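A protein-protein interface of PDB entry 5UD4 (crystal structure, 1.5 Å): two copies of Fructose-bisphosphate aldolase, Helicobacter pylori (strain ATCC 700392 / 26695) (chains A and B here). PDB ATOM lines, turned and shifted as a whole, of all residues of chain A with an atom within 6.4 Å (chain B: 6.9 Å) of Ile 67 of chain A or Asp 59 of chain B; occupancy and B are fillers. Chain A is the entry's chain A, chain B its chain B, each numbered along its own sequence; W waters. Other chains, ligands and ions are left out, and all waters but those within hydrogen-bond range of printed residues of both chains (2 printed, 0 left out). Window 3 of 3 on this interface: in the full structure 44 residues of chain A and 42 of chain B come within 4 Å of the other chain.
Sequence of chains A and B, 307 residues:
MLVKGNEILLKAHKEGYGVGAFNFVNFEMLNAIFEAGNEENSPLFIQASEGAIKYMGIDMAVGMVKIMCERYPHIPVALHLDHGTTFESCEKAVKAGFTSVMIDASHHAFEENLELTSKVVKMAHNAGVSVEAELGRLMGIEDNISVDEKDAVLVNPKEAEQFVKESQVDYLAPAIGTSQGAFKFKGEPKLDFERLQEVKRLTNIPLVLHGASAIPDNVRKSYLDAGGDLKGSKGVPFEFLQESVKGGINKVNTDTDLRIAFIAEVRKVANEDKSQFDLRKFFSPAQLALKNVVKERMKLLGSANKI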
ATOM      1  N   VAL A  62      -7.067  -4.517 -22.198  1.00  0.00           N
ATOM      2  CA  VAL A  62      -8.356  -4.772 -21.567  1.00  0.00           C
ATOM      3  C   VAL A  62      -8.156  -5.341 -20.174  1.00  0.00           C
ATOM      4  O   VAL A  62      -8.815  -4.923 -19.215  1.00  0.00           O
ATOM      5  CB  VAL A  62      -9.189  -5.721 -22.442  1.00  0.00           C
ATOM      6  CG1 VAL A  62     -10.487  -6.049 -21.747  1.00  0.00           C
ATOM      7  CG2 VAL A  62      -9.446  -5.105 -23.826  1.00  0.00           C
ATOM      8  N   GLY A  63      -7.228  -6.283 -20.034  1.00  0.00           N
ATOM      9  CA  GLY A  63      -7.041  -6.930 -18.751  1.00  0.00           C
ATOM     10  C   GLY A  63      -6.630  -5.982 -17.641  1.00  0.00           C
ATOM     11  O   GLY A  63      -7.129  -6.091 -16.521  1.00  0.00           O
ATOM     12  N   MET A  64      -5.704  -5.054 -17.923  1.00  0.00           N
ATOM     13  CA  MET A  64      -5.289  -4.096 -16.903  1.00  0.00           C
ATOM     14  C   MET A  64      -6.438  -3.182 -16.527  1.00  0.00           C
ATOM     15  O   MET A  64      -6.617  -2.857 -15.352  1.00  0.00           O
ATOM     16  CB  MET A  64      -4.096  -3.256 -17.357  1.00  0.00           C
ATOM     17  CG  MET A  64      -2.749  -4.005 -17.436  1.00  0.00           C
ATOM     18  SD  MET A  64      -1.281  -2.939 -17.604  1.00  0.00           S
ATOM     19  CE  MET A  64      -1.733  -2.048 -19.070  1.00  0.00           C
ATOM     20  N   VAL A  65      -7.230  -2.752 -17.506  1.00  0.00           N
ATOM     21  CA  VAL A  65      -8.354  -1.884 -17.195  1.00  0.00           C
ATOM     22  C   VAL A  65      -9.391  -2.621 -16.340  1.00  0.00           C
ATOM     23  O   VAL A  65      -9.945  -2.058 -15.388  1.00  0.00           O
ATOM     24  CB  VAL A  65      -8.959  -1.329 -18.495  1.00  0.00           C
ATOM     25  CG1 VAL A  65     -10.245  -0.558 -18.195  1.00  0.00           C
ATOM     26  CG2 VAL A  65      -7.952  -0.424 -19.223  1.00  0.00           C
ATOM     27  N   LYS A  66      -9.672  -3.893 -16.644  1.00  0.00           N
ATOM     28  CA  LYS A  66     -10.626  -4.640 -15.827  1.00  0.00           C
ATOM     29  C   LYS A  66     -10.147  -4.782 -14.382  1.00  0.00           C
ATOM     30  O   LYS A  66     -10.943  -4.658 -13.442  1.00  0.00           O
ATOM     31  CB  LYS A  66     -10.904  -5.994 -16.466  1.00  0.00           C
ATOM     32  CG  LYS A  66     -11.804  -5.848 -17.697  1.00  0.00           C
ATOM     33  CD  LYS A  66     -12.236  -7.178 -18.267  1.00  0.00           C
ATOM     34  CE  LYS A  66     -13.217  -6.997 -19.435  1.00  0.00           C
ATOM     35  NZ  LYS A  66     -13.725  -8.319 -19.923  1.00  0.00           N
ATOM     36  N   ILE A  67      -8.852  -5.009 -14.184  1.00  0.00           N
ATOM     37  CA  ILE A  67      -8.284  -5.038 -12.835  1.00  0.00           C
ATOM     38  C   ILE A  67      -8.480  -3.694 -12.144  1.00  0.00           C
ATOM     39  O   ILE A  67      -8.861  -3.619 -10.966  1.00  0.00           O
ATOM     40  CB  ILE A  67      -6.795  -5.427 -12.903  1.00  0.00           C
ATOM     41  CG1 ILE A  67      -6.674  -6.864 -13.397  1.00  0.00           C
ATOM     42  CG2 ILE A  67      -6.107  -5.230 -11.544  1.00  0.00           C
ATOM     43  CD1 ILE A  67      -5.308  -7.220 -13.911  1.00  0.00           C
ATOM     44  N   MET A  68      -8.204  -2.607 -12.861  1.00  0.00           N
ATOM     45  CA  MET A  68      -8.344  -1.287 -12.255  1.00  0.00           C
ATOM     46  C   MET A  68      -9.797  -0.981 -11.912  1.00  0.00           C
ATOM     47  O   MET A  68     -10.078  -0.393 -10.870  1.00  0.00           O
ATOM     48  CB  MET A  68      -7.740  -0.235 -13.174  1.00  0.00           C
ATOM     49  CG  MET A  68      -6.222  -0.347 -13.272  1.00  0.00           C
ATOM     50  SD  MET A  68      -5.321  -0.219 -11.699  1.00  0.00           S
ATOM     51  CE  MET A  68      -5.776   1.430 -11.199  1.00  0.00           C
ATOM     52  N   CYS A  69     -10.735  -1.366 -12.783  1.00  0.00           N
ATOM     53  CA  CYS A  69     -12.147  -1.157 -12.475  1.00  0.00           C
ATOM     54  C   CYS A  69     -12.567  -1.923 -11.225  1.00  0.00           C
ATOM     55  O   CYS A  69     -13.348  -1.416 -10.414  1.00  0.00           O
ATOM     56  CB  CYS A  69     -13.005  -1.568 -13.677  1.00  0.00           C
ATOM     57  SG  CYS A  69     -12.841  -0.464 -15.084  1.00  0.00           S
ATOM     58  N   GLU A  70     -12.058  -3.145 -11.047  1.00  0.00           N
ATOM     59  CA  GLU A  70     -12.382  -3.907  -9.845  1.00  0.00           C
ATOM     60  C   GLU A  70     -11.738  -3.298  -8.607  1.00  0.00           C
ATOM     61  O   GLU A  70     -12.252  -3.468  -7.498  1.00  0.00           O
ATOM     62  CB  GLU A  70     -11.947  -5.361 -10.014  1.00  0.00           C
ATOM     63  CG  GLU A  70     -12.731  -6.095 -11.077  1.00  0.00           C
ATOM     64  CD  GLU A  70     -12.223  -7.502 -11.317  1.00  0.00           C
ATOM     65  OE1 GLU A  70     -11.195  -7.881 -10.720  1.00  0.00           O
ATOM     66  OE2 GLU A  70     -12.859  -8.231 -12.110  1.00  0.00           O
ATOM     67  N   ARG A  71     -10.626  -2.581  -8.779  1.00  0.00           N
ATOM     68  CA  ARG A  71     -10.000  -1.896  -7.662  1.00  0.00           C
ATOM     69  C   ARG A  71     -10.816  -0.684  -7.232  1.00  0.00           C
ATOM     70  O   ARG A  71     -10.823  -0.325  -6.050  1.00  0.00           O
ATOM     71  CB  ARG A  71      -8.589  -1.479  -8.080  1.00  0.00           C
ATOM     72  CG  ARG A  71      -7.738  -0.908  -7.000  1.00  0.00           C
ATOM     73  CD  ARG A  71      -6.404  -0.466  -7.558  1.00  0.00           C
ATOM     74  NE  ARG A  71      -5.515  -1.582  -7.899  1.00  0.00           N
ATOM     75  CZ  ARG A  71      -4.238  -1.435  -8.250  1.00  0.00           C
ATOM     76  NH1 ARG A  71      -3.685  -0.238  -8.303  1.00  0.00           N
ATOM     77  NH2 ARG A  71      -3.498  -2.491  -8.539  1.00  0.00           N
ATOM     78  N   TYR A  72     -11.521  -0.057  -8.178  1.00  0.00           N
ATOM     79  CA  TYR A  72     -12.306   1.154  -7.938  1.00  0.00           C
ATOM     80  C   TYR A  72     -13.710   0.955  -8.494  1.00  0.00           C
ATOM     81  O   TYR A  72     -14.119   1.645  -9.441  1.00  0.00           O
ATOM     82  CB  TYR A  72     -11.658   2.368  -8.598  1.00  0.00           C
ATOM     83  CG  TYR A  72     -10.294   2.720  -8.065  1.00  0.00           C
ATOM     84  CD1 TYR A  72      -9.141   2.379  -8.764  1.00  0.00           C
ATOM     85  CD2 TYR A  72     -10.162   3.408  -6.875  1.00  0.00           C
ATOM     86  CE1 TYR A  72      -7.887   2.714  -8.281  1.00  0.00           C
ATOM     87  CE2 TYR A  72      -8.922   3.735  -6.377  1.00  0.00           C
ATOM     88  CZ  TYR A  72      -7.787   3.385  -7.082  1.00  0.00           C
ATOM     89  OH  TYR A  72      -6.563   3.735  -6.588  1.00  0.00           O
ATOM     90  N   ILE B  53       5.143  -5.249  -5.068  1.00  0.00           N
ATOM     91  CA  ILE B  53       3.719  -5.494  -4.844  1.00  0.00           C
ATOM     92  C   ILE B  53       3.021  -4.223  -4.349  1.00  0.00           C
ATOM     93  O   ILE B  53       1.890  -3.921  -4.756  1.00  0.00           O
ATOM     94  CB  ILE B  53       3.539  -6.673  -3.867  1.00  0.00           C
ATOM     95  CG1 ILE B  53       3.924  -7.984  -4.561  1.00  0.00           C
ATOM     96  CG2 ILE B  53       2.109  -6.759  -3.350  1.00  0.00           C
ATOM     97  CD1 ILE B  53       3.999  -9.192  -3.654  1.00  0.00           C
ATOM     98  N   MET B  56       2.700  -1.963  -7.559  1.00  0.00           N
ATOM     99  CA  MET B  56       1.713  -2.423  -8.534  1.00  0.00           C
ATOM    100  C   MET B  56       0.336  -2.608  -7.932  1.00  0.00           C
ATOM    101  O   MET B  56      -0.668  -2.381  -8.619  1.00  0.00           O
ATOM    102  CB  MET B  56       2.149  -3.759  -9.128  1.00  0.00           C
ATOM    103  CG  MET B  56       3.241  -3.656 -10.154  1.00  0.00           C
ATOM    104  SD  MET B  56       3.715  -5.255 -10.833  1.00  0.00           S
ATOM    105  CE  MET B  56       4.681  -5.909  -9.487  1.00  0.00           C
ATOM    106  N   GLY B  57       0.272  -2.977  -6.656  1.00  0.00           N
ATOM    107  CA  GLY B  57      -0.907  -3.566  -6.070  1.00  0.00           C
ATOM    108  C   GLY B  57      -0.891  -5.048  -6.354  1.00  0.00           C
ATOM    109  O   GLY B  57      -0.611  -5.445  -7.484  1.00  0.00           O
ATOM    110  N   ILE B  58      -1.161  -5.889  -5.349  1.00  0.00           N
ATOM    111  CA  ILE B  58      -0.990  -7.323  -5.557  1.00  0.00           C
ATOM    112  C   ILE B  58      -1.979  -7.848  -6.603  1.00  0.00           C
ATOM    113  O   ILE B  58      -1.687  -8.822  -7.313  1.00  0.00           O
ATOM    114  CB  ILE B  58      -1.109  -8.059  -4.204  1.00  0.00           C
ATOM    115  CG1 ILE B  58      -0.454  -9.432  -4.301  1.00  0.00           C
ATOM    116  CG2 ILE B  58      -2.560  -8.175  -3.755  1.00  0.00           C
ATOM    117  CD1 ILE B  58      -0.209 -10.094  -2.944  1.00  0.00           C
ATOM    118  N   ASP B  59      -3.146  -7.207  -6.733  1.00  0.00           N
ATOM    119  CA  ASP B  59      -4.132  -7.608  -7.736  1.00  0.00           C
ATOM    120  C   ASP B  59      -3.608  -7.410  -9.157  1.00  0.00           C
ATOM    121  O   ASP B  59      -3.874  -8.225 -10.055  1.00  0.00           O
ATOM    122  CB  ASP B  59      -5.426  -6.819  -7.510  1.00  0.00           C
ATOM    123  CG  ASP B  59      -5.216  -5.292  -7.451  1.00  0.00           C
ATOM    124  OD1 ASP B  59      -6.136  -4.547  -7.857  1.00  0.00           O
ATOM    125  OD2 ASP B  59      -4.160  -4.813  -6.983  1.00  0.00           O
ATOM    126  N   MET B  60      -2.838  -6.354  -9.374  1.00  0.00           N
ATOM    127  CA  MET B  60      -2.259  -6.114 -10.687  1.00  0.00           C
ATOM    128  C   MET B  60      -1.033  -6.983 -10.936  1.00  0.00           C
ATOM    129  O   MET B  60      -0.815  -7.446 -12.067  1.00  0.00           O
ATOM    130  CB  MET B  60      -1.902  -4.638 -10.834  1.00  0.00           C
ATOM    131  CG  MET B  60      -1.361  -4.240 -12.186  1.00  0.00           C
ATOM    132  SD  MET B  60      -2.575  -4.381 -13.496  1.00  0.00           S
ATOM    133  CE  MET B  60      -3.625  -2.964 -13.134  1.00  0.00           C
ATOM    134  N   ALA B  61      -0.225  -7.220  -9.899  1.00  0.00           N
ATOM    135  CA  ALA B  61       0.924  -8.104 -10.060  1.00  0.00           C
ATOM    136  C   ALA B  61       0.472  -9.479 -10.541  1.00  0.00           C
ATOM    137  O   ALA B  61       0.977 -10.000 -11.540  1.00  0.00           O
ATOM    138  CB  ALA B  61       1.693  -8.199  -8.744  1.00  0.00           C
ATOM    139  N   VAL B  62      -0.493 -10.078  -9.841  1.00  0.00           N
ATOM    140  CA  VAL B  62      -1.004 -11.385 -10.238  1.00  0.00           C
ATOM    141  C   VAL B  62      -1.737 -11.281 -11.558  1.00  0.00           C
ATOM    142  O   VAL B  62      -1.552 -12.117 -12.451  1.00  0.00           O
ATOM    143  CB  VAL B  62      -1.919 -11.973  -9.152  1.00  0.00           C
ATOM    144  CG1 VAL B  62      -2.431 -13.337  -9.596  1.00  0.00           C
ATOM    145  CG2 VAL B  62      -1.177 -12.095  -7.827  1.00  0.00           C
ATOM    146  N   GLY B  63      -2.576 -10.251 -11.703  1.00  0.00           N
ATOM    147  CA  GLY B  63      -3.411 -10.154 -12.890  1.00  0.00           C
ATOM    148  C   GLY B  63      -2.614 -10.047 -14.175  1.00  0.00           C
ATOM    149  O   GLY B  63      -2.951 -10.682 -15.173  1.00  0.00           O
ATOM    150  N   MET B  64      -1.559  -9.231 -14.175  1.00  0.00           N
ATOM    151  CA  MET B  64      -0.725  -9.105 -15.365  1.00  0.00           C
ATOM    152  C   MET B  64      -0.038 -10.422 -15.681  1.00  0.00           C
ATOM    153  O   MET B  64       0.076 -10.807 -16.854  1.00  0.00           O
ATOM    154  CB  MET B  64       0.313  -7.994 -15.203  1.00  0.00           C
ATOM    155  CG  MET B  64      -0.251  -6.573 -15.292  1.00  0.00           C
ATOM    156  SD  MET B  64       1.016  -5.294 -15.479  1.00  0.00           S
ATOM    157  CE  MET B  64       2.058  -5.631 -14.096  1.00  0.00           C
ATOM    158  N   ILE B  67      -2.454 -12.824 -17.334  1.00  0.00           N
ATOM    159  CA  ILE B  67      -2.634 -12.461 -18.739  1.00  0.00           C
ATOM    160  C   ILE B  67      -1.455 -12.949 -19.573  1.00  0.00           C
ATOM    161  O   ILE B  67      -1.635 -13.496 -20.673  1.00  0.00           O
ATOM    162  CB  ILE B  67      -2.816 -10.941 -18.868  1.00  0.00           C
ATOM    163  CG1 ILE B  67      -4.142 -10.537 -18.240  1.00  0.00           C
ATOM    164  CG2 ILE B  67      -2.751 -10.495 -20.338  1.00  0.00           C
ATOM    165  CD1 ILE B  67      -4.245  -9.081 -17.910  1.00  0.00           C
ATOM    166  N   ALA B  96      -3.845 -14.221  -3.024  1.00  0.00           N
ATOM    167  CA  ALA B  96      -3.950 -13.484  -4.278  1.00  0.00           C
ATOM    168  C   ALA B  96      -3.644 -14.328  -5.512  1.00  0.00           C
ATOM    169  O   ALA B  96      -3.989 -13.909  -6.624  1.00  0.00           O
ATOM    170  CB  ALA B  96      -3.028 -12.261  -4.241  1.00  0.00           C
HETATM  171  O   HOH W   1      -8.515  -5.367  -8.805  1.00  0.00           O
HETATM  172  O   HOH W   2      -0.798   0.600  -7.310  1.00  0.00           O
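NH2 of Arg 71 of chain A lies within hydrogen-bond range of O of Met 56 of chain B (2.8 Å).
NH2 of Arg 71 of chain A lies within salt-bridge range of OD2 of Asp 59 of chain B, 2.9 Å away.
The side-chain sulfur of Met 68 of chain A is in hydrogen-bond range of the guanidinium group of Arg 71 of chain A (3.8 Å).
Among the printed residues, pairs that only touch across the chains: Arg 71 of chain A with Met 60 of chain B (3.5 Å), Met 68 of chain A with Met 60 of chain B (3.5 Å), Gly 63 of chain A with Ile 67 of chain B (3.6 Å), Ile 67 of chain A with Gly 63 of chain B (3.6 Å), Ile 67 of chain A with Met 60 of chain B (3.7 Å), Met 64 of chain A with Met 60 of chain B (3.7 Å), Arg 71 of chain A with Gly 57 of chain B (3.7 Å), Ile 67 of chain A with Asp 59 of chain B (3.7 Å) and Met 64 of chain A with Met 64 of chain B (3.9 Å).
Of the printed residues of chain B, Gly 63 of chain A touches Ile 67 (3.6 Å).
Of the printed residues of chain B, Met 64 of chain A touches Met 60 and Met 64.
Of chain B, only Asp 59 (3.7 Å), Met 60 (3.7 Å) and Gly 63 (3.6 Å) come within 4 Å of Ile 67 of chain A.
Of the printed residues of chain A, Gly 57 of chain B touches Arg 71.
Ala 61 of chain B touches none of the printed residues of chain A.
Of the printed residues of chain A, Ile 67 of chain B touches Gly 63 (3.6 Å).
The nearest residue of chain A that does not touch Asp 59 of chain B is Met 68 of chain A (5.8 Å).
Of the 12 printed residues of chain B, 7 touch a printed residue of chain A.
Printed residues of chain B that touch a printed residue of chain A: Met 56, Gly 57, Asp 59, Met 60, Gly 63, Met 64 and Ile 67.
Hydrophobic or aromatic side chains of chain B that line the printed part of chain A: Met 60, Met 64 and Ile 67.
Along chain B the printed residues that touch a printed residue of chain A span positions 56 to 67.
Of the 11 printed residues of chain A, 5 touch a printed residue of chain B.
Hydrophobic or aromatic side chains of chain A that line the printed part of chain B: Met 64, Ile 67 and Met 68.
Among the printed residues, Asp or Glu carboxylates within 4 Å of a Lys or Arg side-chain nitrogen of the other chain: Arg 71 of chain A with Asp 59 of chain B (2.9 Å).
Gly 63 of chain A touches Ile 67 of chain B, and with the chains exchanged Ile 67 of chain A touches Gly 63 of chain B.
Met 64 of chain A touches its own counterpart, Met 64 of chain B.
Of the 11 pairs that touch across the chains among the printed residues, 3 have their exchanged pair printed and touching as well.
Water W1 lies within hydrogen-bond range of OD1 of Asp 59 of chain B, O of Ile 67 of chain A and N of Arg 71 of chain A.
Water W2 lies within hydrogen-bond range of the guanidinium group (NH1) of Arg 71 of chain A (3.2 Å) and the backbone carbonyl oxygen (O) of Met 56 of chain B (3.3 Å).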
